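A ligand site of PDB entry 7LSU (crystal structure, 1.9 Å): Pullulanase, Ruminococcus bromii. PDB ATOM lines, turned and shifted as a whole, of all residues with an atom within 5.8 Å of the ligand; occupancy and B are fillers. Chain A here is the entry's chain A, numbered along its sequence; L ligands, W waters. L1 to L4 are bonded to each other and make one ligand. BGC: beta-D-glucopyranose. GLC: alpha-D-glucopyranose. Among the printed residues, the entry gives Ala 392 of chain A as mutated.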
ATOM      1  N   GLN A 264     -22.102  -4.267  25.752  1.00  0.00           N
ATOM      2  CA  GLN A 264     -22.581  -5.027  24.591  1.00  0.00           C
ATOM      3  C   GLN A 264     -21.803  -4.670  23.313  1.00  0.00           C
ATOM      4  O   GLN A 264     -21.583  -5.535  22.460  1.00  0.00           O
ATOM      5  CB  GLN A 264     -24.076  -4.755  24.375  1.00  0.00           C
ATOM      6  CG  GLN A 264     -24.700  -5.565  23.248  1.00  0.00           C
ATOM      7  CD  GLN A 264     -24.600  -4.897  21.896  1.00  0.00           C
ATOM      8  OE1 GLN A 264     -24.333  -3.701  21.773  1.00  0.00           O
ATOM      9  NE2 GLN A 264     -24.827  -5.683  20.852  1.00  0.00           N
ATOM     10  N   ASN A 276     -15.769   1.468  21.644  1.00  0.00           N
ATOM     11  CA  ASN A 276     -16.970   2.019  22.239  1.00  0.00           C
ATOM     12  C   ASN A 276     -16.656   2.455  23.685  1.00  0.00           C
ATOM     13  O   ASN A 276     -15.866   1.812  24.369  1.00  0.00           O
ATOM     14  CB  ASN A 276     -18.144   1.038  22.192  1.00  0.00           C
ATOM     15  CG  ASN A 276     -19.486   1.733  22.290  1.00  0.00           C
ATOM     16  OD1 ASN A 276     -19.834   2.279  23.341  1.00  0.00           O
ATOM     17  ND2 ASN A 276     -20.250   1.706  21.215  1.00  0.00           N
ATOM     18  N   TRP A 277     -17.279   3.561  24.116  1.00  0.00           N
ATOM     19  CA  TRP A 277     -17.196   4.006  25.509  1.00  0.00           C
ATOM     20  C   TRP A 277     -17.733   2.911  26.438  1.00  0.00           C
ATOM     21  O   TRP A 277     -17.177   2.679  27.509  1.00  0.00           O
ATOM     22  CB  TRP A 277     -17.962   5.323  25.725  1.00  0.00           C
ATOM     23  CG  TRP A 277     -17.319   6.548  25.144  1.00  0.00           C
ATOM     24  CD1 TRP A 277     -16.017   6.719  24.776  1.00  0.00           C
ATOM     25  CD2 TRP A 277     -17.971   7.812  24.918  1.00  0.00           C
ATOM     26  NE1 TRP A 277     -15.823   7.998  24.310  1.00  0.00           N
ATOM     27  CE2 TRP A 277     -16.994   8.686  24.389  1.00  0.00           C
ATOM     28  CE3 TRP A 277     -19.274   8.282  25.101  1.00  0.00           C
ATOM     29  CZ2 TRP A 277     -17.299  10.008  24.035  1.00  0.00           C
ATOM     30  CZ3 TRP A 277     -19.572   9.590  24.753  1.00  0.00           C
ATOM     31  CH2 TRP A 277     -18.597  10.430  24.228  1.00  0.00           C
ATOM     32  N   TYR A 279     -21.313   2.440  27.301  1.00  0.00           N
ATOM     33  CA  TYR A 279     -22.460   2.829  28.123  1.00  0.00           C
ATOM     34  C   TYR A 279     -23.672   1.976  27.705  1.00  0.00           C
ATOM     35  O   TYR A 279     -24.761   2.488  27.468  1.00  0.00           O
ATOM     36  CB  TYR A 279     -22.705   4.338  28.012  1.00  0.00           C
ATOM     37  CG  TYR A 279     -21.629   5.167  28.686  1.00  0.00           C
ATOM     38  CD1 TYR A 279     -21.587   5.280  30.063  1.00  0.00           C
ATOM     39  CD2 TYR A 279     -20.639   5.794  27.952  1.00  0.00           C
ATOM     40  CE1 TYR A 279     -20.603   6.022  30.694  1.00  0.00           C
ATOM     41  CE2 TYR A 279     -19.642   6.543  28.572  1.00  0.00           C
ATOM     42  CZ  TYR A 279     -19.624   6.657  29.942  1.00  0.00           C
ATOM     43  OH  TYR A 279     -18.649   7.382  30.561  1.00  0.00           O
ATOM     44  N   ASP A 280     -23.435   0.655  27.648  1.00  0.00           N
ATOM     45  CA  ASP A 280     -24.356  -0.341  27.071  1.00  0.00           C
ATOM     46  C   ASP A 280     -24.294  -1.604  27.920  1.00  0.00           C
ATOM     47  O   ASP A 280     -23.853  -2.648  27.459  1.00  0.00           O
ATOM     48  CB  ASP A 280     -23.974  -0.645  25.617  1.00  0.00           C
ATOM     49  CG  ASP A 280     -23.887   0.580  24.715  1.00  0.00           C
ATOM     50  OD1 ASP A 280     -24.897   1.305  24.620  1.00  0.00           O
ATOM     51  OD2 ASP A 280     -22.809   0.799  24.125  1.00  0.00           O
ATOM     52  N   ASP A 322     -16.754   4.204  36.639  1.00  0.00           N
ATOM     53  CA  ASP A 322     -17.945   4.704  35.963  1.00  0.00           C
ATOM     54  C   ASP A 322     -18.979   3.572  35.925  1.00  0.00           C
ATOM     55  O   ASP A 322     -18.717   2.512  35.347  1.00  0.00           O
ATOM     56  CB  ASP A 322     -17.587   5.220  34.559  1.00  0.00           C
ATOM     57  CG  ASP A 322     -18.647   6.099  33.914  1.00  0.00           C
ATOM     58  OD1 ASP A 322     -19.844   5.929  34.254  1.00  0.00           O
ATOM     59  OD2 ASP A 322     -18.267   6.943  33.085  1.00  0.00           O
ATOM     60  N   VAL A 324     -23.316   2.441  35.548  1.00  0.00           N
ATOM     61  CA  VAL A 324     -24.422   2.764  34.658  1.00  0.00           C
ATOM     62  C   VAL A 324     -25.628   1.892  35.019  1.00  0.00           C
ATOM     63  O   VAL A 324     -26.120   1.120  34.188  1.00  0.00           O
ATOM     64  CB  VAL A 324     -23.990   2.595  33.181  1.00  0.00           C
ATOM     65  CG1 VAL A 324     -25.048   3.062  32.198  1.00  0.00           C
ATOM     66  CG2 VAL A 324     -22.675   3.298  32.914  1.00  0.00           C
ATOM     67  N   ASN A 326     -28.496   3.057  35.657  1.00  0.00           N
ATOM     68  CA  ASN A 326     -29.676   3.808  35.234  1.00  0.00           C
ATOM     69  C   ASN A 326     -30.394   3.089  34.069  1.00  0.00           C
ATOM     70  O   ASN A 326     -31.592   3.267  33.909  1.00  0.00           O
ATOM     71  CB  ASN A 326     -29.333   5.252  34.869  1.00  0.00           C
ATOM     72  CG  ASN A 326     -28.563   5.383  33.580  1.00  0.00           C
ATOM     73  OD1 ASN A 326     -29.144   5.320  32.498  1.00  0.00           O
ATOM     74  ND2 ASN A 326     -27.255   5.561  33.677  1.00  0.00           N
ATOM     75  N   HIS A 327     -29.649   2.303  33.277  1.00  0.00           N
ATOM     76  CA  HIS A 327     -30.231   1.575  32.139  1.00  0.00           C
ATOM     77  C   HIS A 327     -29.344   0.378  31.761  1.00  0.00           C
ATOM     78  O   HIS A 327     -28.176   0.319  32.144  1.00  0.00           O
ATOM     79  CB  HIS A 327     -30.436   2.514  30.941  1.00  0.00           C
ATOM     80  CG  HIS A 327     -29.217   2.732  30.111  1.00  0.00           C
ATOM     81  ND1 HIS A 327     -28.260   3.665  30.442  1.00  0.00           N
ATOM     82  CD2 HIS A 327     -28.790   2.127  28.984  1.00  0.00           C
ATOM     83  CE1 HIS A 327     -27.292   3.640  29.545  1.00  0.00           C
ATOM     84  NE2 HIS A 327     -27.592   2.704  28.639  1.00  0.00           N
ATOM     85  N   TYR A 329     -28.417  -2.185  28.119  1.00  0.00           N
ATOM     86  CA  TYR A 329     -28.331  -2.047  26.656  1.00  0.00           C
ATOM     87  C   TYR A 329     -29.714  -2.248  26.020  1.00  0.00           C
ATOM     88  O   TYR A 329     -30.121  -1.478  25.143  1.00  0.00           O
ATOM     89  CB  TYR A 329     -27.336  -3.032  26.042  1.00  0.00           C
ATOM     90  CG  TYR A 329     -27.384  -3.084  24.534  1.00  0.00           C
ATOM     91  CD1 TYR A 329     -26.975  -1.997  23.778  1.00  0.00           C
ATOM     92  CD2 TYR A 329     -27.881  -4.181  23.867  1.00  0.00           C
ATOM     93  CE1 TYR A 329     -27.025  -2.018  22.390  1.00  0.00           C
ATOM     94  CE2 TYR A 329     -27.943  -4.228  22.475  1.00  0.00           C
ATOM     95  CZ  TYR A 329     -27.518  -3.140  21.738  1.00  0.00           C
ATOM     96  OH  TYR A 329     -27.576  -3.172  20.380  1.00  0.00           O
ATOM     97  N   SER A 356     -33.439   7.467  30.147  1.00  0.00           N
ATOM     98  CA  SER A 356     -32.023   7.329  29.813  1.00  0.00           C
ATOM     99  C   SER A 356     -31.730   7.873  28.415  1.00  0.00           C
ATOM    100  O   SER A 356     -30.636   8.365  28.154  1.00  0.00           O
ATOM    101  CB  SER A 356     -31.584   5.887  29.926  1.00  0.00           C
ATOM    102  OG  SER A 356     -32.196   5.092  28.914  1.00  0.00           O
ATOM    103  N   GLY A 357     -32.730   7.786  27.522  1.00  0.00           N
ATOM    104  CA  GLY A 357     -32.571   8.072  26.106  1.00  0.00           C
ATOM    105  C   GLY A 357     -31.981   6.887  25.356  1.00  0.00           C
ATOM    106  O   GLY A 357     -31.591   7.018  24.192  1.00  0.00           O
ATOM    107  N   CYS A 358     -31.932   5.729  26.022  1.00  0.00           N
ATOM    108  CA  CYS A 358     -31.315   4.504  25.497  1.00  0.00           C
ATOM    109  C   CYS A 358     -32.336   3.363  25.393  1.00  0.00           C
ATOM    110  O   CYS A 358     -31.979   2.267  24.947  1.00  0.00           O
ATOM    111  CB  CYS A 358     -30.140   4.085  26.377  1.00  0.00           C
ATOM    112  SG  CYS A 358     -28.798   5.304  26.391  1.00  0.00           S
ATOM    113  N   GLY A 359     -33.585   3.603  25.822  1.00  0.00           N
ATOM    114  CA  GLY A 359     -34.706   2.677  25.581  1.00  0.00           C
ATOM    115  C   GLY A 359     -35.380   2.196  26.858  1.00  0.00           C
ATOM    116  O   GLY A 359     -36.483   1.658  26.803  1.00  0.00           O
ATOM    117  N   ARG A 390     -18.437   6.926  39.828  1.00  0.00           N
ATOM    118  CA  ARG A 390     -19.130   7.973  39.082  1.00  0.00           C
ATOM    119  C   ARG A 390     -20.425   7.384  38.512  1.00  0.00           C
ATOM    120  O   ARG A 390     -20.387   6.436  37.734  1.00  0.00           O
ATOM    121  CB  ARG A 390     -18.223   8.538  37.979  1.00  0.00           C
ATOM    122  CG  ARG A 390     -18.900   9.545  37.047  1.00  0.00           C
ATOM    123  CD  ARG A 390     -19.389   8.950  35.744  1.00  0.00           C
ATOM    124  NE  ARG A 390     -19.725   9.976  34.770  1.00  0.00           N
ATOM    125  CZ  ARG A 390     -20.454   9.783  33.667  1.00  0.00           C
ATOM    126  NH1 ARG A 390     -20.946   8.591  33.404  1.00  0.00           N
ATOM    127  NH2 ARG A 390     -20.683  10.787  32.846  1.00  0.00           N
ATOM    128  N   PHE A 391     -21.564   7.964  38.906  1.00  0.00           N
ATOM    129  CA  PHE A 391     -22.885   7.462  38.532  1.00  0.00           C
ATOM    130  C   PHE A 391     -23.377   8.173  37.275  1.00  0.00           C
ATOM    131  O   PHE A 391     -23.653   9.373  37.285  1.00  0.00           O
ATOM    132  CB  PHE A 391     -23.875   7.653  39.693  1.00  0.00           C
ATOM    133  CG  PHE A 391     -23.591   6.779  40.880  1.00  0.00           C
ATOM    134  CD1 PHE A 391     -22.757   7.221  41.900  1.00  0.00           C
ATOM    135  CD2 PHE A 391     -24.138   5.514  40.973  1.00  0.00           C
ATOM    136  CE1 PHE A 391     -22.483   6.408  42.988  1.00  0.00           C
ATOM    137  CE2 PHE A 391     -23.871   4.702  42.072  1.00  0.00           C
ATOM    138  CZ  PHE A 391     -23.049   5.152  43.076  1.00  0.00           C
ATOM    139  N   ALA A 392     -23.468   7.398  36.181  1.00  0.00           N
ATOM    140  CA  ALA A 392     -24.075   7.850  34.934  1.00  0.00           C
ATOM    141  C   ALA A 392     -25.552   8.171  35.159  1.00  0.00           C
ATOM    142  O   ALA A 392     -26.261   7.377  35.783  1.00  0.00           O
ATOM    143  CB  ALA A 392     -23.896   6.796  33.875  1.00  0.00           C
ATOM    144  N   LEU A 393     -25.995   9.332  34.651  1.00  0.00           N
ATOM    145  CA  LEU A 393     -27.359   9.831  34.809  1.00  0.00           C
ATOM    146  C   LEU A 393     -27.883   9.499  36.214  1.00  0.00           C
ATOM    147  O   LEU A 393     -28.833   8.726  36.366  1.00  0.00           O
ATOM    148  CB  LEU A 393     -28.254   9.225  33.725  1.00  0.00           C
ATOM    149  CG  LEU A 393     -27.820   9.470  32.277  1.00  0.00           C
ATOM    150  CD1 LEU A 393     -28.847   8.909  31.306  1.00  0.00           C
ATOM    151  CD2 LEU A 393     -27.605  10.947  32.011  1.00  0.00           C
ATOM    152  N   GLU A 421     -23.702  12.585  37.399  1.00  0.00           N
ATOM    153  CA  GLU A 421     -24.462  13.545  36.616  1.00  0.00           C
ATOM    154  C   GLU A 421     -25.805  13.785  37.298  1.00  0.00           C
ATOM    155  O   GLU A 421     -26.619  12.857  37.408  1.00  0.00           O
ATOM    156  CB  GLU A 421     -24.706  13.019  35.203  1.00  0.00           C
ATOM    157  CG  GLU A 421     -23.456  12.896  34.353  1.00  0.00           C
ATOM    158  CD  GLU A 421     -23.699  12.147  33.051  1.00  0.00           C
ATOM    159  OE1 GLU A 421     -23.351  12.682  31.983  1.00  0.00           O
ATOM    160  OE2 GLU A 421     -24.247  11.029  33.112  1.00  0.00           O
ATOM    161  N   HIS A 518     -15.443  13.347  28.790  1.00  0.00           N
ATOM    162  CA  HIS A 518     -15.451  12.480  27.602  1.00  0.00           C
ATOM    163  C   HIS A 518     -16.583  12.890  26.641  1.00  0.00           C
ATOM    164  O   HIS A 518     -16.435  12.759  25.435  1.00  0.00           O
ATOM    165  CB  HIS A 518     -15.553  11.001  28.014  1.00  0.00           C
ATOM    166  CG  HIS A 518     -16.907  10.588  28.489  1.00  0.00           C
ATOM    167  ND1 HIS A 518     -17.294  10.690  29.811  1.00  0.00           N
ATOM    168  CD2 HIS A 518     -17.968  10.083  27.824  1.00  0.00           C
ATOM    169  CE1 HIS A 518     -18.542  10.261  29.934  1.00  0.00           C
ATOM    170  NE2 HIS A 518     -18.974   9.882  28.725  1.00  0.00           N
ATOM    171  N   ASP A 519     -17.704  13.365  27.197  1.00  0.00           N
ATOM    172  CA  ASP A 519     -18.853  13.816  26.412  1.00  0.00           C
ATOM    173  C   ASP A 519     -18.520  15.139  25.715  1.00  0.00           C
ATOM    174  O   ASP A 519     -17.662  15.892  26.172  1.00  0.00           O
ATOM    175  CB  ASP A 519     -20.106  14.005  27.275  1.00  0.00           C
ATOM    176  CG  ASP A 519     -20.833  12.705  27.598  1.00  0.00           C
ATOM    177  OD1 ASP A 519     -21.151  11.970  26.641  1.00  0.00           O
ATOM    178  OD2 ASP A 519     -21.088  12.455  28.788  1.00  0.00           O
ATOM    179  N   ASN A 578     -19.255  13.672  19.918  1.00  0.00           N
ATOM    180  CA  ASN A 578     -19.873  12.479  20.502  1.00  0.00           C
ATOM    181  C   ASN A 578     -19.151  11.255  19.950  1.00  0.00           C
ATOM    182  O   ASN A 578     -19.657  10.550  19.082  1.00  0.00           O
ATOM    183  CB  ASN A 578     -21.390  12.437  20.229  1.00  0.00           C
ATOM    184  CG  ASN A 578     -22.118  11.416  21.070  1.00  0.00           C
ATOM    185  OD1 ASN A 578     -21.655  11.037  22.148  1.00  0.00           O
ATOM    186  ND2 ASN A 578     -23.258  10.956  20.592  1.00  0.00           N
ATOM    187  N   TYR A 580     -18.380   8.287  20.826  1.00  0.00           N
ATOM    188  CA  TYR A 580     -18.649   7.089  21.620  1.00  0.00           C
ATOM    189  C   TYR A 580     -18.377   5.809  20.821  1.00  0.00           C
ATOM    190  O   TYR A 580     -17.997   4.799  21.409  1.00  0.00           O
ATOM    191  CB  TYR A 580     -20.073   7.113  22.200  1.00  0.00           C
ATOM    192  CG  TYR A 580     -21.200   6.850  21.222  1.00  0.00           C
ATOM    193  CD1 TYR A 580     -21.714   7.866  20.440  1.00  0.00           C
ATOM    194  CD2 TYR A 580     -21.794   5.606  21.131  1.00  0.00           C
ATOM    195  CE1 TYR A 580     -22.761   7.655  19.562  1.00  0.00           C
ATOM    196  CE2 TYR A 580     -22.843   5.363  20.257  1.00  0.00           C
ATOM    197  CZ  TYR A 580     -23.331   6.389  19.473  1.00  0.00           C
ATOM    198  OH  TYR A 580     -24.362   6.180  18.613  1.00  0.00           O
HETATM  199  C2  BGC L   1     -22.462   9.280  29.599  1.00  0.00           C
HETATM  200  C3  BGC L   1     -22.745   9.453  28.110  1.00  0.00           C
HETATM  201  C4  BGC L   1     -23.710   8.376  27.629  1.00  0.00           C
HETATM  202  C5  BGC L   1     -24.958   8.373  28.516  1.00  0.00           C
HETATM  203  C6  BGC L   1     -25.978   7.327  28.080  1.00  0.00           C
HETATM  204  C1  BGC L   1     -23.756   9.200  30.386  1.00  0.00           C
HETATM  205  O1  BGC L   1     -23.445   8.953  31.752  1.00  0.00           O
HETATM  206  O2  BGC L   1     -21.659  10.362  30.088  1.00  0.00           O
HETATM  207  O3  BGC L   1     -21.508   9.407  27.391  1.00  0.00           O
HETATM  208  O4  BGC L   1     -24.099   8.591  26.269  1.00  0.00           O
HETATM  209  O5  BGC L   1     -24.584   8.155  29.867  1.00  0.00           O
HETATM  210  O6  BGC L   1     -27.055   7.253  29.017  1.00  0.00           O
HETATM  211  C1  GLC L   2     -23.254   7.886  25.343  1.00  0.00           C
HETATM  212  C2  GLC L   2     -23.310   8.579  23.990  1.00  0.00           C
HETATM  213  C3  GLC L   2     -24.684   8.375  23.352  1.00  0.00           C
HETATM  214  C4  GLC L   2     -25.035   6.898  23.290  1.00  0.00           C
HETATM  215  C5  GLC L   2     -24.897   6.253  24.669  1.00  0.00           C
HETATM  216  C6  GLC L   2     -25.141   4.748  24.635  1.00  0.00           C
HETATM  217  O2  GLC L   2     -23.046   9.973  24.154  1.00  0.00           O
HETATM  218  O3  GLC L   2     -24.702   8.947  22.042  1.00  0.00           O
HETATM  219  O4  GLC L   2     -26.403   6.777  22.853  1.00  0.00           O
HETATM  220  O5  GLC L   2     -23.587   6.499  25.202  1.00  0.00           O
HETATM  221  O6  GLC L   2     -24.125   4.089  23.875  1.00  0.00           O
HETATM  222  C1  GLC L   3     -26.540   6.098  21.589  1.00  0.00           C
HETATM  223  C2  GLC L   3     -27.511   6.878  20.703  1.00  0.00           C
HETATM  224  C3  GLC L   3     -28.920   6.828  21.288  1.00  0.00           C
HETATM  225  C4  GLC L   3     -29.327   5.384  21.530  1.00  0.00           C
HETATM  226  C5  GLC L   3     -28.284   4.686  22.388  1.00  0.00           C
HETATM  227  C6  GLC L   3     -28.619   3.218  22.645  1.00  0.00           C
HETATM  228  O2  GLC L   3     -27.075   8.239  20.585  1.00  0.00           O
HETATM  229  O3  GLC L   3     -29.846   7.458  20.387  1.00  0.00           O
HETATM  230  O4  GLC L   3     -30.613   5.362  22.162  1.00  0.00           O
HETATM  231  O5  GLC L   3     -27.012   4.758  21.748  1.00  0.00           O
HETATM  232  O6  GLC L   3     -28.595   2.521  21.392  1.00  0.00           O
HETATM  233  C1  GLC L   4     -29.154   1.201  21.528  1.00  0.00           C
HETATM  234  C2  GLC L   4     -28.964   0.460  20.208  1.00  0.00           C
HETATM  235  C3  GLC L   4     -29.799   1.106  19.109  1.00  0.00           C
HETATM  236  C4  GLC L   4     -31.255   1.217  19.547  1.00  0.00           C
HETATM  237  C5  GLC L   4     -31.363   1.881  20.921  1.00  0.00           C
HETATM  238  C6  GLC L   4     -32.798   1.919  21.434  1.00  0.00           C
HETATM  239  O2  GLC L   4     -27.578   0.482  19.848  1.00  0.00           O
HETATM  240  O3  GLC L   4     -29.708   0.351  17.906  1.00  0.00           O
HETATM  241  O4  GLC L   4     -31.996   1.960  18.575  1.00  0.00           O
HETATM  242  O5  GLC L   4     -30.548   1.196  21.871  1.00  0.00           O
HETATM  243  O6  GLC L   4     -33.280   0.577  21.647  1.00  0.00           O
HETATM  244  O   HOH W   1     -21.521   4.149  24.839  1.00  0.00           O
HETATM  245  O   HOH W   2     -30.338   5.810  18.055  1.00  0.00           O
HETATM  246  O   HOH W   3     -26.379   8.538  17.989  1.00  0.00           O
HETATM  247  O   HOH W   4     -31.092  -1.755  22.608  1.00  0.00           O
HETATM  248  O   HOH W   5     -22.957   2.153  21.553  1.00  0.00           O
HETATM  249  O   HOH W   6     -25.778   2.553  20.601  1.00  0.00           O
HETATM  250  O   HOH W   7     -26.066   6.233  31.195  1.00  0.00           O
HETATM  251  O   HOH W   8     -28.279   9.496  27.611  1.00  0.00           O
HETATM  252  O   HOH W   9     -24.691  11.508  25.714  1.00  0.00           O
HETATM  253  O   HOH W  10     -29.386   0.929  24.837  1.00  0.00           O
HETATM  254  O   HOH W  11     -26.355  -1.649  18.666  1.00  0.00           O
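O1 of BGC L1 is in hydrogen-bond range of OE2 of Glu 421. NH2 of Arg 390 is in hydrogen-bond range of O2 of BGC L1, 3.0 Å away. SG of Cys 358 sits at hydrogen-bond distance from O6 of BGC L1, 3.7 Å away. The backbone carbonyl oxygen of Gly 357 is in hydrogen-bond range of an oxygen (O4) of GLC L3 (2.8 Å). OD1 of Asn 578 lies within hydrogen-bond range of O2 of GLC L2, 2.7 Å away. The side-chain carboxylate (OD2) of Asp 519 lies within hydrogen-bond range of an oxygen (O2) of BGC L1, 2.5 Å away. O6 of GLC L2 sits at hydrogen-bond distance from OD1 of Asp 280. NE2 of His 518 lies within hydrogen-bond range of O3 of BGC L1 (2.9 Å).
OD1 of Asp 322 is in salt-bridge range of NH1 of Arg 390, at 3.0 Å. The backbone carbonyl oxygen (O) of Tyr 279 sits at hydrogen-bond distance from a ring nitrogen (NE2) of His 327 (3.1 Å). The backbone carbonyl oxygen (O) of Asp 280 sits at hydrogen-bond distance from the backbone NH (N) of Gln 264, at 2.9 Å. The guanidinium group (NH2) of Arg 390 lies within salt-bridge range of the side-chain carboxylate (OE1) of Glu 421, at 3.4 Å. A ring nitrogen (NE2) of His 518 sits at hydrogen-bond distance from the side-chain carboxylate (OD2) of Asp 519 (3.3 Å). The backbone carbonyl oxygen of Ala 392 sits at hydrogen-bond distance from the side-chain amide nitrogen of Asn 326 (3.0 Å). O of Tyr 580 sits at hydrogen-bond distance from N of Trp 277, 3.1 Å away. The side-chain hydroxyl (OH) of Tyr 279 lies within hydrogen-bond range of the side-chain carboxylate (OD2) of Asp 322 (2.6 Å).
Merely in contact with the ligand: Ala 392 (3.1 Å), Trp 277 (3.3 Å), Leu 393 (3.3 Å), Tyr 580 (3.4 Å), Tyr 329 (3.6 Å), Tyr 279 (3.6 Å), His 327 (3.7 Å) and Ser 356 (3.8 Å). Hydrophobic or aromatic side chains that line the ligand: Trp 277, Tyr 279, His 327, Tyr 329, Ala 392, Leu 393, His 518 and Tyr 580. Within 4 Å of the ligand: Trp 277, Tyr 279, Asp 280, His 327, Tyr 329, Ser 356, Gly 357, Cys 358, Arg 390, Ala 392, Leu 393, Glu 421, His 518, Asp 519, Asn 578 and Tyr 580. The nearest printed residue that does not touch the ligand is Asn 326 (4.5 Å).
Water W3 bridges an oxygen (O2) of GLC L3 and the side-chain hydroxyl of Tyr 580. Water W11 lies within hydrogen-bond range of the side-chain hydroxyl of Tyr 329 (2.6 Å) and an oxygen (O2) of GLC L4 (2.7 Å). Water W1 lies within hydrogen-bond range of O6 of GLC L2 (2.8 Å), OD1 of Asn 276 (2.9 Å) and N of Tyr 279 (3.0 Å). Water W8 lies within hydrogen-bond range of O of Ser 356 (2.7 Å) and O6 of BGC L1 (2.9 Å). Water W4 bridges the backbone carbonyl oxygen of Tyr 329 (2.7 Å) and an oxygen (O5) of GLC L4 (3.1 Å). Water W5 lies within hydrogen-bond range of the side-chain amide nitrogen of Asn 276 (2.8 Å), the side-chain carboxylate of Asp 280 (2.9 Å) and an oxygen (O6) of GLC L2 (3.2 Å).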
